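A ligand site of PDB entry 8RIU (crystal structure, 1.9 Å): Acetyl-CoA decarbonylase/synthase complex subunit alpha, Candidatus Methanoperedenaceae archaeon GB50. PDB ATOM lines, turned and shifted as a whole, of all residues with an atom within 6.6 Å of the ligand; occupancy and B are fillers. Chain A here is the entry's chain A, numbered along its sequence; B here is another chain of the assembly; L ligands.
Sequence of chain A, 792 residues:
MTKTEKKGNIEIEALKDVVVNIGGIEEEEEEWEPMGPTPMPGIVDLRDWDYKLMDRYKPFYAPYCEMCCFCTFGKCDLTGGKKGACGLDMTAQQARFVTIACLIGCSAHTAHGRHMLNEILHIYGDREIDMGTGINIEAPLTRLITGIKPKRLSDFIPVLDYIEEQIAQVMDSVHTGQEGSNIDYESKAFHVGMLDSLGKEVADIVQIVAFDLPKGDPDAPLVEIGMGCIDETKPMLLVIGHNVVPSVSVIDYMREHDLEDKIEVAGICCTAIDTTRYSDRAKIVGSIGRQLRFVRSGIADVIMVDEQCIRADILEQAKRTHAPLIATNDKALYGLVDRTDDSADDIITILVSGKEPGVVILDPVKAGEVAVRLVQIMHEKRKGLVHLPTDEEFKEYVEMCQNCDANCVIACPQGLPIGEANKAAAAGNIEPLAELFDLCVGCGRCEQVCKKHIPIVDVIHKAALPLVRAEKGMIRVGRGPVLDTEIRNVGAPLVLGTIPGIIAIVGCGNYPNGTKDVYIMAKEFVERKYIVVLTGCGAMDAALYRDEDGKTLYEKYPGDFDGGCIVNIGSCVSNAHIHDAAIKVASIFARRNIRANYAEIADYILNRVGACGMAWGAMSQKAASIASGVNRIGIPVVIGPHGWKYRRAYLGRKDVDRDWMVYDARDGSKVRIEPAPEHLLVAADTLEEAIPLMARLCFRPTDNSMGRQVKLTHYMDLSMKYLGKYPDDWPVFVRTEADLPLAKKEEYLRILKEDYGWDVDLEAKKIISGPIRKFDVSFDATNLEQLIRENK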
ATOM      1  N   HIS A 109     -23.970 -19.642 -16.229  1.00  0.00           N
ATOM      2  CA  HIS A 109     -24.484 -19.752 -17.585  1.00  0.00           C
ATOM      3  C   HIS A 109     -25.907 -20.265 -17.586  1.00  0.00           C
ATOM      4  O   HIS A 109     -26.787 -19.726 -18.274  1.00  0.00           O
ATOM      5  CB  HIS A 109     -23.570 -20.673 -18.410  1.00  0.00           C
ATOM      6  CG  HIS A 109     -22.240 -20.065 -18.724  1.00  0.00           C
ATOM      7  ND1 HIS A 109     -21.054 -20.751 -18.590  1.00  0.00           N
ATOM      8  CD2 HIS A 109     -21.923 -18.835 -19.183  1.00  0.00           C
ATOM      9  CE1 HIS A 109     -20.052 -19.964 -18.925  1.00  0.00           C
ATOM     10  NE2 HIS A 109     -20.555 -18.796 -19.302  1.00  0.00           N
ATOM     11  N   GLY A 241     -21.818  -6.317 -18.309  1.00  0.00           N
ATOM     12  CA  GLY A 241     -22.322  -7.577 -17.802  1.00  0.00           C
ATOM     13  C   GLY A 241     -22.389  -8.640 -18.877  1.00  0.00           C
ATOM     14  O   GLY A 241     -21.547  -8.669 -19.788  1.00  0.00           O
ATOM     15  N   HIS A 242     -23.422  -9.488 -18.800  1.00  0.00           N
ATOM     16  CA  HIS A 242     -23.584 -10.613 -19.772  1.00  0.00           C
ATOM     17  C   HIS A 242     -25.029 -10.737 -20.257  1.00  0.00           C
ATOM     18  O   HIS A 242     -25.218 -11.277 -21.359  1.00  0.00           O
ATOM     19  CB  HIS A 242     -23.170 -11.926 -19.112  1.00  0.00           C
ATOM     20  CG  HIS A 242     -21.704 -12.063 -19.017  1.00  0.00           C
ATOM     21  ND1 HIS A 242     -20.930 -11.322 -18.156  1.00  0.00           N
ATOM     22  CD2 HIS A 242     -20.876 -12.838 -19.702  1.00  0.00           C
ATOM     23  CE1 HIS A 242     -19.670 -11.655 -18.323  1.00  0.00           C
ATOM     24  NE2 HIS A 242     -19.615 -12.573 -19.263  1.00  0.00           N
ATOM     25  N   CYS A 269     -17.348  -6.151 -21.608  1.00  0.00           N
ATOM     26  CA  CYS A 269     -17.620  -7.576 -21.423  1.00  0.00           C
ATOM     27  C   CYS A 269     -18.797  -8.005 -22.289  1.00  0.00           C
ATOM     28  O   CYS A 269     -19.228  -7.259 -23.162  1.00  0.00           O
ATOM     29  CB  CYS A 269     -17.845  -7.897 -19.947  1.00  0.00           C
ATOM     30  SG  CYS A 269     -16.364  -7.608 -18.924  1.00  0.00           S
ATOM     31  N   CYS A 270     -19.332  -9.209 -22.052  1.00  0.00           N
ATOM     32  CA  CYS A 270     -20.125  -9.871 -23.091  1.00  0.00           C
ATOM     33  C   CYS A 270     -21.421  -9.139 -23.440  1.00  0.00           C
ATOM     34  O   CYS A 270     -21.924  -9.319 -24.545  1.00  0.00           O
ATOM     35  CB  CYS A 270     -20.439 -11.296 -22.668  1.00  0.00           C
ATOM     36  SG  CYS A 270     -19.008 -12.330 -22.959  1.00  0.00           S
ATOM     37  N   THR A 271     -21.992  -8.348 -22.529  1.00  0.00           N
ATOM     38  CA  THR A 271     -23.175  -7.597 -22.931  1.00  0.00           C
ATOM     39  C   THR A 271     -22.879  -6.743 -24.140  1.00  0.00           C
ATOM     40  O   THR A 271     -23.767  -6.503 -24.972  1.00  0.00           O
ATOM     41  CB  THR A 271     -23.686  -6.746 -21.766  1.00  0.00           C
ATOM     42  OG1 THR A 271     -24.275  -7.597 -20.776  1.00  0.00           O
ATOM     43  CG2 THR A 271     -24.751  -5.762 -22.247  1.00  0.00           C
ATOM     44  N   SER A 287     -12.514  -5.298 -23.046  1.00  0.00           N
ATOM     45  CA  SER A 287     -12.587  -6.479 -22.156  1.00  0.00           C
ATOM     46  C   SER A 287     -12.559  -6.118 -20.668  1.00  0.00           C
ATOM     47  O   SER A 287     -12.544  -4.925 -20.350  1.00  0.00           O
ATOM     48  CB  SER A 287     -11.439  -7.391 -22.493  1.00  0.00           C
ATOM     49  OG  SER A 287     -10.253  -6.646 -22.724  1.00  0.00           O
ATOM     50  N   ILE A 288     -12.508  -7.133 -19.799  1.00  0.00           N
ATOM     51  CA  ILE A 288     -12.532  -6.923 -18.322  1.00  0.00           C
ATOM     52  C   ILE A 288     -11.373  -6.025 -17.898  1.00  0.00           C
ATOM     53  O   ILE A 288     -11.597  -5.142 -17.077  1.00  0.00           O
ATOM     54  CB  ILE A 288     -12.497  -8.282 -17.591  1.00  0.00           C
ATOM     55  CG1 ILE A 288     -12.492  -8.121 -16.072  1.00  0.00           C
ATOM     56  CG2 ILE A 288     -11.317  -9.115 -18.070  1.00  0.00           C
ATOM     57  CD1 ILE A 288     -13.834  -7.714 -15.506  1.00  0.00           C
ATOM     58  N   GLN A 308     -22.496 -10.688 -13.733  1.00  0.00           N
ATOM     59  CA  GLN A 308     -21.242 -11.379 -14.163  1.00  0.00           C
ATOM     60  C   GLN A 308     -20.133 -10.464 -14.685  1.00  0.00           C
ATOM     61  O   GLN A 308     -20.385  -9.699 -15.627  1.00  0.00           O
ATOM     62  CB  GLN A 308     -21.582 -12.478 -15.177  1.00  0.00           C
ATOM     63  CG  GLN A 308     -22.522 -13.536 -14.621  1.00  0.00           C
ATOM     64  CD  GLN A 308     -23.001 -14.501 -15.688  1.00  0.00           C
ATOM     65  OE1 GLN A 308     -22.377 -14.630 -16.737  1.00  0.00           O
ATOM     66  NE2 GLN A 308     -24.103 -15.162 -15.421  1.00  0.00           N
ATOM     67  N   CYS A 309     -18.933 -10.562 -14.092  1.00  0.00           N
ATOM     68  CA  CYS A 309     -17.733  -9.825 -14.570  1.00  0.00           C
ATOM     69  C   CYS A 309     -17.898  -8.304 -14.449  1.00  0.00           C
ATOM     70  O   CYS A 309     -17.198  -7.579 -15.172  1.00  0.00           O
ATOM     71  CB  CYS A 309     -17.378 -10.304 -15.976  1.00  0.00           C
ATOM     72  SG  CYS A 309     -17.287 -12.116 -16.043  1.00  0.00           S
ATOM     73  N   VAL A 506     -10.201 -17.914 -26.657  1.00  0.00           N
ATOM     74  CA  VAL A 506     -11.372 -17.518 -25.846  1.00  0.00           C
ATOM     75  C   VAL A 506     -10.914 -17.158 -24.433  1.00  0.00           C
ATOM     76  O   VAL A 506      -9.711 -17.214 -24.168  1.00  0.00           O
ATOM     77  CB  VAL A 506     -12.354 -18.698 -25.766  1.00  0.00           C
ATOM     78  CG1 VAL A 506     -12.699 -19.261 -27.140  1.00  0.00           C
ATOM     79  CG2 VAL A 506     -11.821 -19.806 -24.865  1.00  0.00           C
ATOM     80  N   GLY A 507     -11.866 -16.784 -23.601  1.00  0.00           N
ATOM     81  CA  GLY A 507     -11.542 -16.590 -22.187  1.00  0.00           C
ATOM     82  C   GLY A 507     -11.292 -15.172 -21.767  1.00  0.00           C
ATOM     83  O   GLY A 507     -11.356 -14.277 -22.622  1.00  0.00           O
ATOM     84  N   CYS A 508     -10.933 -15.011 -20.505  1.00  0.00           N
ATOM     85  CA  CYS A 508     -10.804 -13.673 -19.892  1.00  0.00           C
ATOM     86  C   CYS A 508      -9.483 -12.972 -20.219  1.00  0.00           C
ATOM     87  O   CYS A 508      -8.658 -13.555 -20.932  1.00  0.00           O
ATOM     88  CB  CYS A 508     -10.962 -13.810 -18.384  1.00  0.00           C
ATOM     89  SG  CYS A 508     -12.042 -15.187 -17.881  1.00  0.00           S
ATOM     90  N   GLY A 509      -9.312 -11.771 -19.674  1.00  0.00           N
ATOM     91  CA  GLY A 509      -8.137 -10.957 -19.991  1.00  0.00           C
ATOM     92  C   GLY A 509      -7.129 -10.830 -18.863  1.00  0.00           C
ATOM     93  O   GLY A 509      -6.464  -9.801 -18.810  1.00  0.00           O
ATOM     94  N   THR A 535     -14.073 -15.763 -29.004  1.00  0.00           N
ATOM     95  CA  THR A 535     -15.265 -15.403 -28.207  1.00  0.00           C
ATOM     96  C   THR A 535     -14.875 -14.531 -27.017  1.00  0.00           C
ATOM     97  O   THR A 535     -13.686 -14.473 -26.698  1.00  0.00           O
ATOM     98  CB  THR A 535     -15.957 -16.636 -27.596  1.00  0.00           C
ATOM     99  OG1 THR A 535     -15.052 -17.258 -26.688  1.00  0.00           O
ATOM    100  CG2 THR A 535     -16.422 -17.632 -28.639  1.00  0.00           C
ATOM    101  N   GLY A 536     -15.862 -13.865 -26.430  1.00  0.00           N
ATOM    102  CA  GLY A 536     -15.644 -13.101 -25.207  1.00  0.00           C
ATOM    103  C   GLY A 536     -14.487 -12.122 -25.280  1.00  0.00           C
ATOM    104  O   GLY A 536     -14.229 -11.500 -26.314  1.00  0.00           O
ATOM    105  N   CYS A 537     -13.770 -12.005 -24.171  1.00  0.00           N
ATOM    106  CA  CYS A 537     -12.709 -11.011 -24.090  1.00  0.00           C
ATOM    107  C   CYS A 537     -11.607 -11.275 -25.110  1.00  0.00           C
ATOM    108  O   CYS A 537     -11.009 -10.322 -25.627  1.00  0.00           O
ATOM    109  CB  CYS A 537     -12.136 -10.965 -22.662  1.00  0.00           C
ATOM    110  SG  CYS A 537     -13.305 -10.325 -21.438  1.00  0.00           S
ATOM    111  N   GLY A 538     -11.315 -12.538 -25.410  1.00  0.00           N
ATOM    112  CA  GLY A 538     -10.317 -12.823 -26.422  1.00  0.00           C
ATOM    113  C   GLY A 538     -10.659 -12.204 -27.757  1.00  0.00           C
ATOM    114  O   GLY A 538      -9.819 -11.545 -28.378  1.00  0.00           O
ATOM    115  N   SER A 571     -20.332 -14.109 -27.710  1.00  0.00           N
ATOM    116  CA  SER A 571     -20.043 -13.925 -26.298  1.00  0.00           C
ATOM    117  C   SER A 571     -19.622 -15.252 -25.676  1.00  0.00           C
ATOM    118  O   SER A 571     -19.525 -16.286 -26.345  1.00  0.00           O
ATOM    119  CB  SER A 571     -21.258 -13.339 -25.595  1.00  0.00           C
ATOM    120  OG  SER A 571     -22.420 -14.097 -25.886  1.00  0.00           O
ATOM    121  N   CYS A 572     -19.376 -15.236 -24.364  1.00  0.00           N
ATOM    122  CA  CYS A 572     -18.883 -16.442 -23.702  1.00  0.00           C
ATOM    123  C   CYS A 572     -19.875 -17.593 -23.798  1.00  0.00           C
ATOM    124  O   CYS A 572     -19.460 -18.751 -23.887  1.00  0.00           O
ATOM    125  CB  CYS A 572     -18.544 -16.133 -22.238  1.00  0.00           C
ATOM    126  SG  CYS A 572     -17.007 -15.186 -22.000  1.00  0.00           S
ATOM    127  N   VAL A 573     -21.180 -17.306 -23.792  1.00  0.00           N
ATOM    128  CA  VAL A 573     -22.163 -18.366 -24.005  1.00  0.00           C
ATOM    129  C   VAL A 573     -22.090 -18.905 -25.429  1.00  0.00           C
ATOM    130  O   VAL A 573     -22.445 -20.059 -25.683  1.00  0.00           O
ATOM    131  CB  VAL A 573     -23.592 -17.895 -23.657  1.00  0.00           C
ATOM    132  CG1 VAL A 573     -23.763 -17.721 -22.145  1.00  0.00           C
ATOM    133  CG2 VAL A 573     -23.935 -16.612 -24.417  1.00  0.00           C
ATOM    134  N   ASN A 575     -19.589 -19.848 -26.886  1.00  0.00           N
ATOM    135  CA  ASN A 575     -18.587 -20.898 -26.967  1.00  0.00           C
ATOM    136  C   ASN A 575     -19.225 -22.234 -27.356  1.00  0.00           C
ATOM    137  O   ASN A 575     -18.628 -23.029 -28.085  1.00  0.00           O
ATOM    138  CB  ASN A 575     -17.854 -21.046 -25.629  1.00  0.00           C
ATOM    139  CG  ASN A 575     -16.724 -20.050 -25.473  1.00  0.00           C
ATOM    140  OD1 ASN A 575     -15.890 -19.875 -26.360  1.00  0.00           O
ATOM    141  ND2 ASN A 575     -16.687 -19.383 -24.323  1.00  0.00           N
ATOM    142  N   GLY A 617      -5.786 -15.691 -20.932  1.00  0.00           N
ATOM    143  CA  GLY A 617      -6.019 -14.922 -19.723  1.00  0.00           C
ATOM    144  C   GLY A 617      -7.099 -15.506 -18.829  1.00  0.00           C
ATOM    145  O   GLY A 617      -7.759 -14.772 -18.102  1.00  0.00           O
ATOM    146  N   ALA A 618      -7.275 -16.833 -18.874  1.00  0.00           N
ATOM    147  CA  ALA A 618      -8.318 -17.487 -18.091  1.00  0.00           C
ATOM    148  C   ALA A 618      -8.279 -17.013 -16.647  1.00  0.00           C
ATOM    149  O   ALA A 618      -7.218 -16.979 -16.008  1.00  0.00           O
ATOM    150  CB  ALA A 618      -8.144 -19.013 -18.156  1.00  0.00           C
ATOM    151  N   MET A 619      -9.455 -16.634 -16.138  1.00  0.00           N
ATOM    152  CA  MET A 619      -9.592 -16.007 -14.820  1.00  0.00           C
ATOM    153  C   MET A 619     -10.805 -16.493 -14.026  1.00  0.00           C
ATOM    154  O   MET A 619     -10.665 -16.907 -12.881  1.00  0.00           O
ATOM    155  CB  MET A 619      -9.653 -14.479 -15.016  1.00  0.00           C
ATOM    156  CG  MET A 619      -9.888 -13.610 -13.764  1.00  0.00           C
ATOM    157  SD  MET A 619     -11.614 -13.587 -13.217  1.00  0.00           S
ATOM    158  CE  MET A 619     -12.303 -12.382 -14.337  1.00  0.00           C
ATOM    159  N   SER A 620     -11.980 -16.459 -14.635  1.00  0.00           N
ATOM    160  CA  SER A 620     -13.239 -16.591 -13.922  1.00  0.00           C
ATOM    161  C   SER A 620     -13.546 -18.047 -13.568  1.00  0.00           C
ATOM    162  O   SER A 620     -12.855 -18.981 -13.971  1.00  0.00           O
ATOM    163  CB  SER A 620     -14.386 -16.049 -14.762  1.00  0.00           C
ATOM    164  OG  SER A 620     -14.387 -16.648 -16.042  1.00  0.00           O
ATOM    165  N   GLN A 621     -14.627 -18.219 -12.793  1.00  0.00           N
ATOM    166  CA  GLN A 621     -15.178 -19.559 -12.600  1.00  0.00           C
ATOM    167  C   GLN A 621     -15.862 -20.045 -13.872  1.00  0.00           C
ATOM    168  O   GLN A 621     -15.841 -21.251 -14.168  1.00  0.00           O
ATOM    169  CB  GLN A 621     -16.152 -19.569 -11.428  1.00  0.00           C
ATOM    170  CG  GLN A 621     -15.563 -19.117 -10.108  1.00  0.00           C
ATOM    171  CD  GLN A 621     -15.512 -17.609  -9.965  1.00  0.00           C
ATOM    172  OE1 GLN A 621     -16.418 -16.898 -10.399  1.00  0.00           O
ATOM    173  NE2 GLN A 621     -14.436 -17.114  -9.365  1.00  0.00           N
ATOM    174  N   LYS A 622     -16.457 -19.130 -14.627  1.00  0.00           N
ATOM    175  CA  LYS A 622     -17.002 -19.498 -15.926  1.00  0.00           C
ATOM    176  C   LYS A 622     -15.917 -20.009 -16.861  1.00  0.00           C
ATOM    177  O   LYS A 622     -16.187 -20.890 -17.689  1.00  0.00           O
ATOM    178  CB  LYS A 622     -17.719 -18.300 -16.547  1.00  0.00           C
ATOM    179  CG  LYS A 622     -19.171 -18.139 -16.039  1.00  0.00           C
ATOM    180  CD  LYS A 622     -19.865 -16.881 -16.573  1.00  0.00           C
ATOM    181  CE  LYS A 622     -19.223 -15.582 -16.130  1.00  0.00           C
ATOM    182  NZ  LYS A 622     -19.310 -14.520 -17.213  1.00  0.00           N
ATOM    183  N   ALA A 623     -14.684 -19.504 -16.744  1.00  0.00           N
ATOM    184  CA  ALA A 623     -13.623 -19.999 -17.603  1.00  0.00           C
ATOM    185  C   ALA A 623     -13.219 -21.427 -17.230  1.00  0.00           C
ATOM    186  O   ALA A 623     -12.872 -22.226 -18.100  1.00  0.00           O
ATOM    187  CB  ALA A 623     -12.413 -19.071 -17.565  1.00  0.00           C
ATOM    188  N   ILE A 626     -16.053 -23.688 -18.599  1.00  0.00           N
ATOM    189  CA  ILE A 626     -15.900 -23.748 -20.049  1.00  0.00           C
ATOM    190  C   ILE A 626     -14.827 -24.772 -20.426  1.00  0.00           C
ATOM    191  O   ILE A 626     -15.044 -25.657 -21.256  1.00  0.00           O
ATOM    192  CB  ILE A 626     -15.572 -22.355 -20.612  1.00  0.00           C
ATOM    193  CG1 ILE A 626     -16.808 -21.468 -20.536  1.00  0.00           C
ATOM    194  CG2 ILE A 626     -15.094 -22.448 -22.044  1.00  0.00           C
ATOM    195  CD1 ILE A 626     -16.514 -20.000 -20.679  1.00  0.00           C
ATOM    196  N   HIS B 175     -20.420 -15.874  -8.318  1.00  0.00           N
ATOM    197  CA  HIS B 175     -19.390 -15.735  -9.382  1.00  0.00           C
ATOM    198  C   HIS B 175     -18.725 -14.372  -9.232  1.00  0.00           C
ATOM    199  O   HIS B 175     -19.332 -13.426  -8.727  1.00  0.00           O
ATOM    200  CB  HIS B 175     -19.987 -15.885 -10.785  1.00  0.00           C
ATOM    201  CG  HIS B 175     -18.967 -16.008 -11.867  1.00  0.00           C
ATOM    202  ND1 HIS B 175     -18.266 -14.944 -12.363  1.00  0.00           N
ATOM    203  CD2 HIS B 175     -18.538 -17.080 -12.541  1.00  0.00           C
ATOM    204  CE1 HIS B 175     -17.441 -15.363 -13.301  1.00  0.00           C
ATOM    205  NE2 HIS B 175     -17.585 -16.660 -13.427  1.00  0.00           N
HETATM  206 FE1  LIG L   1     -14.524 -11.899 -20.260  1.00  0.00          FE
HETATM  207 FE2  LIG L   1     -17.936 -12.934 -20.769  1.00  0.00          FE
HETATM  208 FE3  LIG L   1     -13.947 -14.117 -18.589  1.00  0.00          FE
HETATM  209 FE4  LIG L   1     -16.090 -12.433 -17.864  1.00  0.00          FE
HETATM  210  S1  LIG L   1     -15.849 -14.612 -17.831  1.00  0.00           S
HETATM  211  S2  LIG L   1     -14.266 -12.253 -18.210  1.00  0.00           S
HETATM  212  S3  LIG L   1     -14.385 -13.926 -20.516  1.00  0.00           S
HETATM  213  S4  LIG L   1     -16.435 -11.655 -19.811  1.00  0.00           S
HETATM  214 NI1  LIG L   1     -16.252 -14.875 -20.164  1.00  0.00          NI
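The side-chain sulfur (SG) of Cys 572 is bound to a nickel atom (NI1) of the ligand.
SG of Cys 309 binds FE4 of the ligand (2.2 Å).
A ring nitrogen (NE2) of His 242 is bound to an iron atom (FE2) of the ligand, 2.3 Å away.
The backbone NH (N) of Cys 508 lies close to a sulfur (S3) of the ligand (3.6 Å).
SG of Cys 508 binds FE3 of the ligand.
An iron atom (FE1) of the ligand is bound by the side-chain sulfur (SG) of Cys 537, 2.3 Å away.
An iron atom (FE2) of the ligand is bound by the side-chain sulfur (SG) of Cys 270, at 2.5 Å.
OG of Ser 620 lies close to S1 of the ligand.
NZ of Lys 622 lies close to S1 of the ligand (3.5 Å).
A ring nitrogen (NE2) of His 242 lies close to the side-chain amino group of Lys 622 (2.8 Å).
The side-chain sulfur (SG) of Cys 508 lies close to the backbone NH (N) of Met 619, at 3.4 Å.
The backbone NH (N) of Ile 288 lies close to the side-chain sulfur (SG) of Cys 537 (3.7 Å).
The backbone carbonyl oxygen of Gly 241 sits at hydrogen-bond distance from the backbone NH of Cys 270.
The backbone NH of Ala 623 is in hydrogen-bond range of the side-chain hydroxyl of Ser 620.
The backbone NH (N) of Lys 622 lies within hydrogen-bond range of a ring nitrogen (NE2) of His 175 of chain B, at 3.0 Å.
The side-chain amino group (NZ) of Lys 622 sits at hydrogen-bond distance from the side-chain amide oxygen (OE1) of Gln 308.
The backbone carbonyl oxygen of Gly 507 sits at hydrogen-bond distance from the backbone NH of Gly 538, at 3.3 Å.
A sulfur (S3) of the ligand lies close to the backbone carbonyl oxygen of Gly 507, at 3.7 Å.
Hydrophobic or aromatic side chains within 4 Å of the ligand: His 242.
Nine residues have an atom within 4 Å of the ligand: His 242, Cys 270, Cys 309, Gly 507, Cys 508, Cys 537, Cys 572, Ser 620 and Lys 622.
Along chain A the residues within 4 Å of the ligand span positions 242 to 622.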
